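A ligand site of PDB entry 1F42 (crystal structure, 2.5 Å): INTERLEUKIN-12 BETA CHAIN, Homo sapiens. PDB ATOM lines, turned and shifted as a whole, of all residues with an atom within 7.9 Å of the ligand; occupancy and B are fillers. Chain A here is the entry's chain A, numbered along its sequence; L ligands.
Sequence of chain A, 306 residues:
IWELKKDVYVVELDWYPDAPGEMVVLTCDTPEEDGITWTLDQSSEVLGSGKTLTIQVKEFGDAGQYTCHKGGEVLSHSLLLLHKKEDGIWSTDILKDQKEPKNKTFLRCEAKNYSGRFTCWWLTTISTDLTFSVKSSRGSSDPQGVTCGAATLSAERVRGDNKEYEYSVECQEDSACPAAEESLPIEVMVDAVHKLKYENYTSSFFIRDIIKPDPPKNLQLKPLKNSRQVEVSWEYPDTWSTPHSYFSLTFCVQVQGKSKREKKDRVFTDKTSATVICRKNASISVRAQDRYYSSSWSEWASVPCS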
ATOM      1  N   PHE A 251      25.967  -1.220 -24.320  1.00  0.00           N
ATOM      2  CA  PHE A 251      25.271  -1.793 -23.194  1.00  0.00           C
ATOM      3  C   PHE A 251      23.811  -1.995 -23.453  1.00  0.00           C
ATOM      4  O   PHE A 251      23.167  -1.286 -24.238  1.00  0.00           O
ATOM      5  CB  PHE A 251      25.424  -0.863 -21.939  1.00  0.00           C
ATOM      6  CG  PHE A 251      26.843  -0.593 -21.548  1.00  0.00           C
ATOM      7  CD1 PHE A 251      27.563  -1.524 -20.784  1.00  0.00           C
ATOM      8  CD2 PHE A 251      27.510   0.555 -22.031  1.00  0.00           C
ATOM      9  CE1 PHE A 251      28.962  -1.323 -20.508  1.00  0.00           C
ATOM     10  CE2 PHE A 251      28.907   0.773 -21.770  1.00  0.00           C
ATOM     11  CZ  PHE A 251      29.629  -0.183 -21.007  1.00  0.00           C
ATOM     12  N   CYS A 252      23.312  -2.971 -22.698  1.00  0.00           N
ATOM     13  CA  CYS A 252      21.812  -3.133 -22.627  1.00  0.00           C
ATOM     14  C   CYS A 252      21.230  -3.114 -21.199  1.00  0.00           C
ATOM     15  O   CYS A 252      21.713  -3.620 -20.299  1.00  0.00           O
ATOM     16  CB  CYS A 252      21.525  -4.374 -23.704  1.00  0.00           C
ATOM     17  SG  CYS A 252      19.719  -4.660 -23.740  1.00  0.00           S
ATOM     18  N   VAL A 253      20.246  -2.250 -20.980  1.00  0.00           N
ATOM     19  CA  VAL A 253      19.448  -1.975 -19.528  1.00  0.00           C
ATOM     20  C   VAL A 253      18.074  -2.606 -19.601  1.00  0.00           C
ATOM     21  O   VAL A 253      17.383  -2.512 -20.624  1.00  0.00           O
ATOM     22  CB  VAL A 253      19.457  -0.450 -19.194  1.00  0.00           C
ATOM     23  CG1 VAL A 253      19.012  -0.256 -17.772  1.00  0.00           C
ATOM     24  CG2 VAL A 253      20.857   0.152 -19.437  1.00  0.00           C
ATOM     25  N   GLN A 254      17.740  -3.336 -18.534  1.00  0.00           N
ATOM     26  CA  GLN A 254      16.474  -4.032 -18.401  1.00  0.00           C
ATOM     27  C   GLN A 254      15.976  -3.925 -16.960  1.00  0.00           C
ATOM     28  O   GLN A 254      16.769  -3.979 -16.016  1.00  0.00           O
ATOM     29  CB  GLN A 254      16.696  -5.496 -18.767  1.00  0.00           C
ATOM     30  CG  GLN A 254      15.445  -6.312 -19.062  1.00  0.00           C
ATOM     31  CD  GLN A 254      15.751  -7.800 -19.240  1.00  0.00           C
ATOM     32  OE1 GLN A 254      15.554  -8.598 -18.314  1.00  0.00           O
ATOM     33  NE2 GLN A 254      16.273  -8.173 -20.422  1.00  0.00           N
ATOM     34  N   VAL A 255      14.655  -3.802 -16.810  1.00  0.00           N
ATOM     35  CA  VAL A 255      14.041  -3.735 -15.483  1.00  0.00           C
ATOM     36  C   VAL A 255      13.441  -5.149 -15.223  1.00  0.00           C
ATOM     37  O   VAL A 255      12.496  -5.573 -15.887  1.00  0.00           O
ATOM     38  CB  VAL A 255      12.981  -2.557 -15.356  1.00  0.00           C
ATOM     39  CG1 VAL A 255      12.580  -2.348 -13.914  1.00  0.00           C
ATOM     40  CG2 VAL A 255      13.566  -1.250 -15.879  1.00  0.00           C
ATOM     41  N   GLN A 256      14.102  -5.914 -14.348  1.00  0.00           N
ATOM     42  CA  GLN A 256      13.690  -7.289 -14.003  1.00  0.00           C
ATOM     43  C   GLN A 256      12.712  -7.300 -12.820  1.00  0.00           C
ATOM     44  O   GLN A 256      13.132  -7.122 -11.674  1.00  0.00           O
ATOM     45  CB  GLN A 256      14.936  -8.168 -13.688  1.00  0.00           C
ATOM     46  CG  GLN A 256      16.056  -8.172 -14.769  1.00  0.00           C
ATOM     47  CD  GLN A 256      16.945  -9.438 -14.721  1.00  0.00           C
ATOM     48  OE1 GLN A 256      16.509 -10.539 -15.079  1.00  0.00           O
ATOM     49  NE2 GLN A 256      18.204  -9.276 -14.306  1.00  0.00           N
ATOM     50  N   ARG A 266      13.822  -3.408 -22.334  1.00  0.00           N
ATOM     51  CA  ARG A 266      15.086  -3.485 -23.063  1.00  0.00           C
ATOM     52  C   ARG A 266      15.493  -2.188 -23.735  1.00  0.00           C
ATOM     53  O   ARG A 266      14.835  -1.738 -24.680  1.00  0.00           O
ATOM     54  CB  ARG A 266      15.064  -4.587 -24.130  1.00  0.00           C
ATOM     55  CG  ARG A 266      15.381  -5.978 -23.640  1.00  0.00           C
ATOM     56  CD  ARG A 266      15.878  -6.779 -24.820  1.00  0.00           C
ATOM     57  NE  ARG A 266      15.761  -8.221 -24.642  1.00  0.00           N
ATOM     58  CZ  ARG A 266      16.565  -9.116 -25.224  1.00  0.00           C
ATOM     59  NH1 ARG A 266      16.380 -10.413 -25.009  1.00  0.00           N
ATOM     60  NH2 ARG A 266      17.598  -8.709 -25.971  1.00  0.00           N
ATOM     61  N   VAL A 267      16.577  -1.577 -23.223  1.00  0.00           N
ATOM     62  CA  VAL A 267      17.129  -0.321 -23.749  1.00  0.00           C
ATOM     63  C   VAL A 267      18.613  -0.536 -24.105  1.00  0.00           C
ATOM     64  O   VAL A 267      19.375  -1.040 -23.303  1.00  0.00           O
ATOM     65  CB  VAL A 267      16.919   0.863 -22.723  1.00  0.00           C
ATOM     66  CG1 VAL A 267      17.731   2.110 -23.088  1.00  0.00           C
ATOM     67  CG2 VAL A 267      15.453   1.237 -22.639  1.00  0.00           C
ATOM     68  N   PHE A 268      18.997  -0.127 -25.313  1.00  0.00           N
ATOM     69  CA  PHE A 268      20.364  -0.231 -25.840  1.00  0.00           C
ATOM     70  C   PHE A 268      21.028   1.129 -25.829  1.00  0.00           C
ATOM     71  O   PHE A 268      20.422   2.093 -26.273  1.00  0.00           O
ATOM     72  CB  PHE A 268      20.328  -0.780 -27.287  1.00  0.00           C
ATOM     73  CG  PHE A 268      19.924  -2.202 -27.367  1.00  0.00           C
ATOM     74  CD1 PHE A 268      20.911  -3.221 -27.354  1.00  0.00           C
ATOM     75  CD2 PHE A 268      18.558  -2.565 -27.323  1.00  0.00           C
ATOM     76  CE1 PHE A 268      20.528  -4.611 -27.281  1.00  0.00           C
ATOM     77  CE2 PHE A 268      18.155  -3.945 -27.250  1.00  0.00           C
ATOM     78  CZ  PHE A 268      19.146  -4.976 -27.231  1.00  0.00           C
ATOM     79  N   SER A 285      18.938  -4.076 -14.479  1.00  0.00           N
ATOM     80  CA  SER A 285      20.061  -4.910 -14.892  1.00  0.00           C
ATOM     81  C   SER A 285      20.766  -4.379 -16.144  1.00  0.00           C
ATOM     82  O   SER A 285      20.114  -3.830 -17.020  1.00  0.00           O
ATOM     83  CB  SER A 285      19.619  -6.358 -15.056  1.00  0.00           C
ATOM     84  OG  SER A 285      19.504  -6.959 -13.785  1.00  0.00           O
ATOM     85  N   VAL A 286      22.094  -4.495 -16.182  1.00  0.00           N
ATOM     86  CA  VAL A 286      22.931  -3.991 -17.283  1.00  0.00           C
ATOM     87  C   VAL A 286      23.999  -5.007 -17.753  1.00  0.00           C
ATOM     88  O   VAL A 286      24.738  -5.570 -16.943  1.00  0.00           O
ATOM     89  CB  VAL A 286      23.691  -2.683 -16.861  1.00  0.00           C
ATOM     90  CG1 VAL A 286      24.332  -1.979 -18.152  1.00  0.00           C
ATOM     91  CG2 VAL A 286      22.767  -1.702 -16.076  1.00  0.00           C
ATOM     92  N   ARG A 287      24.087  -5.207 -19.052  1.00  0.00           N
ATOM     93  CA  ARG A 287      25.056  -6.123 -19.694  1.00  0.00           C
ATOM     94  C   ARG A 287      25.916  -5.323 -20.683  1.00  0.00           C
ATOM     95  O   ARG A 287      25.464  -4.270 -21.187  1.00  0.00           O
ATOM     96  CB  ARG A 287      24.302  -7.166 -20.532  1.00  0.00           C
ATOM     97  CG  ARG A 287      23.960  -8.462 -19.947  1.00  0.00           C
ATOM     98  CD  ARG A 287      23.163  -9.285 -20.992  1.00  0.00           C
ATOM     99  NE  ARG A 287      22.339 -10.344 -20.397  1.00  0.00           N
ATOM    100  CZ  ARG A 287      22.742 -11.562 -20.022  1.00  0.00           C
ATOM    101  NH1 ARG A 287      23.999 -11.961 -20.166  1.00  0.00           N
ATOM    102  NH2 ARG A 287      21.878 -12.379 -19.421  1.00  0.00           N
ATOM    103  N   ALA A 288      27.034  -5.924 -21.097  1.00  0.00           N
ATOM    104  CA  ALA A 288      27.992  -5.329 -22.030  1.00  0.00           C
ATOM    105  C   ALA A 288      28.430  -6.270 -23.129  1.00  0.00           C
ATOM    106  O   ALA A 288      28.642  -7.474 -22.927  1.00  0.00           O
ATOM    107  CB  ALA A 288      29.292  -4.775 -21.279  1.00  0.00           C
ATOM    108  N   GLN A 289      28.679  -5.645 -24.278  1.00  0.00           N
ATOM    109  CA  GLN A 289      29.117  -6.320 -25.462  1.00  0.00           C
ATOM    110  C   GLN A 289      30.109  -5.415 -26.144  1.00  0.00           C
ATOM    111  O   GLN A 289      29.970  -4.203 -26.085  1.00  0.00           O
ATOM    112  CB  GLN A 289      27.941  -6.508 -26.424  1.00  0.00           C
ATOM    113  CG  GLN A 289      28.173  -7.458 -27.584  1.00  0.00           C
ATOM    114  CD  GLN A 289      26.960  -7.594 -28.514  1.00  0.00           C
ATOM    115  OE1 GLN A 289      26.328  -6.606 -28.893  1.00  0.00           O
ATOM    116  NE2 GLN A 289      26.619  -8.819 -28.867  1.00  0.00           N
ATOM    117  N   SER A 296      29.788 -12.418 -27.260  1.00  0.00           N
ATOM    118  CA  SER A 296      28.957 -12.663 -26.096  1.00  0.00           C
ATOM    119  C   SER A 296      28.719 -11.477 -25.218  1.00  0.00           C
ATOM    120  O   SER A 296      29.592 -10.609 -25.059  1.00  0.00           O
ATOM    121  CB  SER A 296      29.528 -13.780 -25.206  1.00  0.00           C
ATOM    122  OG  SER A 296      29.353 -15.056 -25.765  1.00  0.00           O
ATOM    123  N   TRP A 297      27.474 -11.418 -24.742  1.00  0.00           N
ATOM    124  CA  TRP A 297      27.034 -10.428 -23.794  1.00  0.00           C
ATOM    125  C   TRP A 297      27.575 -10.925 -22.437  1.00  0.00           C
ATOM    126  O   TRP A 297      27.607 -12.155 -22.148  1.00  0.00           O
ATOM    127  CB  TRP A 297      25.516 -10.323 -23.733  1.00  0.00           C
ATOM    128  CG  TRP A 297      24.890  -9.574 -24.867  1.00  0.00           C
ATOM    129  CD1 TRP A 297      24.366 -10.108 -26.017  1.00  0.00           C
ATOM    130  CD2 TRP A 297      24.779  -8.140 -25.006  1.00  0.00           C
ATOM    131  NE1 TRP A 297      23.960  -9.111 -26.869  1.00  0.00           N
ATOM    132  CE2 TRP A 297      24.176  -7.890 -26.283  1.00  0.00           C
ATOM    133  CE3 TRP A 297      25.109  -7.043 -24.185  1.00  0.00           C
ATOM    134  CZ2 TRP A 297      23.907  -6.570 -26.764  1.00  0.00           C
ATOM    135  CZ3 TRP A 297      24.855  -5.713 -24.657  1.00  0.00           C
ATOM    136  CH2 TRP A 297      24.252  -5.500 -25.942  1.00  0.00           C
ATOM    137  N   SER A 298      28.042  -9.975 -21.637  1.00  0.00           N
ATOM    138  CA  SER A 298      28.556 -10.259 -20.310  1.00  0.00           C
ATOM    139  C   SER A 298      27.412 -10.764 -19.413  1.00  0.00           C
ATOM    140  O   SER A 298      26.268 -10.682 -19.779  1.00  0.00           O
ATOM    141  CB  SER A 298      29.088  -8.958 -19.697  1.00  0.00           C
ATOM    142  OG  SER A 298      28.028  -8.101 -19.325  1.00  0.00           O
ATOM    143  N   GLU A 299      27.756 -11.195 -18.203  1.00  0.00           N
ATOM    144  CA  GLU A 299      26.795 -11.593 -17.195  1.00  0.00           C
ATOM    145  C   GLU A 299      26.159 -10.257 -16.710  1.00  0.00           C
ATOM    146  O   GLU A 299      26.740  -9.161 -16.892  1.00  0.00           O
ATOM    147  CB  GLU A 299      27.540 -12.285 -16.032  1.00  0.00           C
ATOM    148  CG  GLU A 299      28.051 -13.738 -16.346  1.00  0.00           C
ATOM    149  CD  GLU A 299      26.881 -14.667 -16.776  1.00  0.00           C
ATOM    150  OE1 GLU A 299      25.891 -14.773 -16.002  1.00  0.00           O
ATOM    151  OE2 GLU A 299      26.874 -15.189 -17.929  1.00  0.00           O
ATOM    152  N   TRP A 300      24.934 -10.331 -16.184  1.00  0.00           N
ATOM    153  CA  TRP A 300      24.277  -9.147 -15.648  1.00  0.00           C
ATOM    154  C   TRP A 300      24.935  -8.543 -14.398  1.00  0.00           C
ATOM    155  O   TRP A 300      25.556  -9.248 -13.559  1.00  0.00           O
ATOM    156  CB  TRP A 300      22.854  -9.485 -15.229  1.00  0.00           C
ATOM    157  CG  TRP A 300      21.858  -9.821 -16.305  1.00  0.00           C
ATOM    158  CD1 TRP A 300      21.195 -11.006 -16.442  1.00  0.00           C
ATOM    159  CD2 TRP A 300      21.287  -8.932 -17.299  1.00  0.00           C
ATOM    160  NE1 TRP A 300      20.241 -10.917 -17.435  1.00  0.00           N
ATOM    161  CE2 TRP A 300      20.267  -9.660 -17.976  1.00  0.00           C
ATOM    162  CE3 TRP A 300      21.528  -7.590 -17.674  1.00  0.00           C
ATOM    163  CZ2 TRP A 300      19.482  -9.092 -19.020  1.00  0.00           C
ATOM    164  CZ3 TRP A 300      20.746  -7.010 -18.710  1.00  0.00           C
ATOM    165  CH2 TRP A 300      19.730  -7.767 -19.367  1.00  0.00           C
HETATM  166  C1  LIG L   1      19.020  -8.895 -22.606  1.00  0.00           C
HETATM  167  C2  LIG L   1      19.445 -10.202 -23.005  1.00  0.00           C
HETATM  168  C3  LIG L   1      20.590 -10.333 -23.809  1.00  0.00           C
HETATM  169  C4  LIG L   1      21.287  -9.199 -24.221  1.00  0.00           C
HETATM  170  C5  LIG L   1      20.856  -7.884 -23.819  1.00  0.00           C
HETATM  171  C6  LIG L   1      19.737  -7.735 -23.010  1.00  0.00           C
HETATM  172  S1  LIG L   1      19.251  -6.077 -22.351  1.00  0.00           S
HETATM  173  C7  LIG L   1      18.707 -11.353 -22.638  1.00  0.00           C
HETATM  174  O1  LIG L   1      17.960 -11.899 -23.491  1.00  0.00           O
HETATM  175  O2  LIG L   1      18.809 -11.841 -21.468  1.00  0.00           O
HETATM  176  N1  LIG L   1      21.123 -11.653 -24.114  1.00  0.00           N
HETATM  177  O3  LIG L   1      21.916 -12.355 -23.237  1.00  0.00           O
HETATM  178  O4  LIG L   1      20.884 -12.307 -25.298  1.00  0.00           O
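A sulfur (S1) of the ligand is covalently linked to the side-chain sulfur of Cys 252, 2.0 Å away. NH1 of Arg 266 lies within salt-bridge range of O1 of the ligand, at 2.6 Å. The guanidinium group (NH2) of Arg 287 lies within salt-bridge range of an oxygen (O2) of the ligand (3.7 Å).
The indole nitrogen (NE1) of Trp 297 sits close to the side-chain amide nitrogen (NE2) of Gln 289, 3.3 Å away. O of Arg 287 lies within hydrogen-bond range of N of Cys 252 (2.9 Å). NH1 of Arg 287 lies within hydrogen-bond range of O of Ser 298. N of Ser 285 lies within hydrogen-bond range of O of Gln 254.
Residues that only touch the ligand: Trp 300 (3.5 Å), Gln 254 (3.6 Å) and Trp 297 (3.7 Å). Of the 19 residues printed, 6 come within 4 Å of the ligand.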
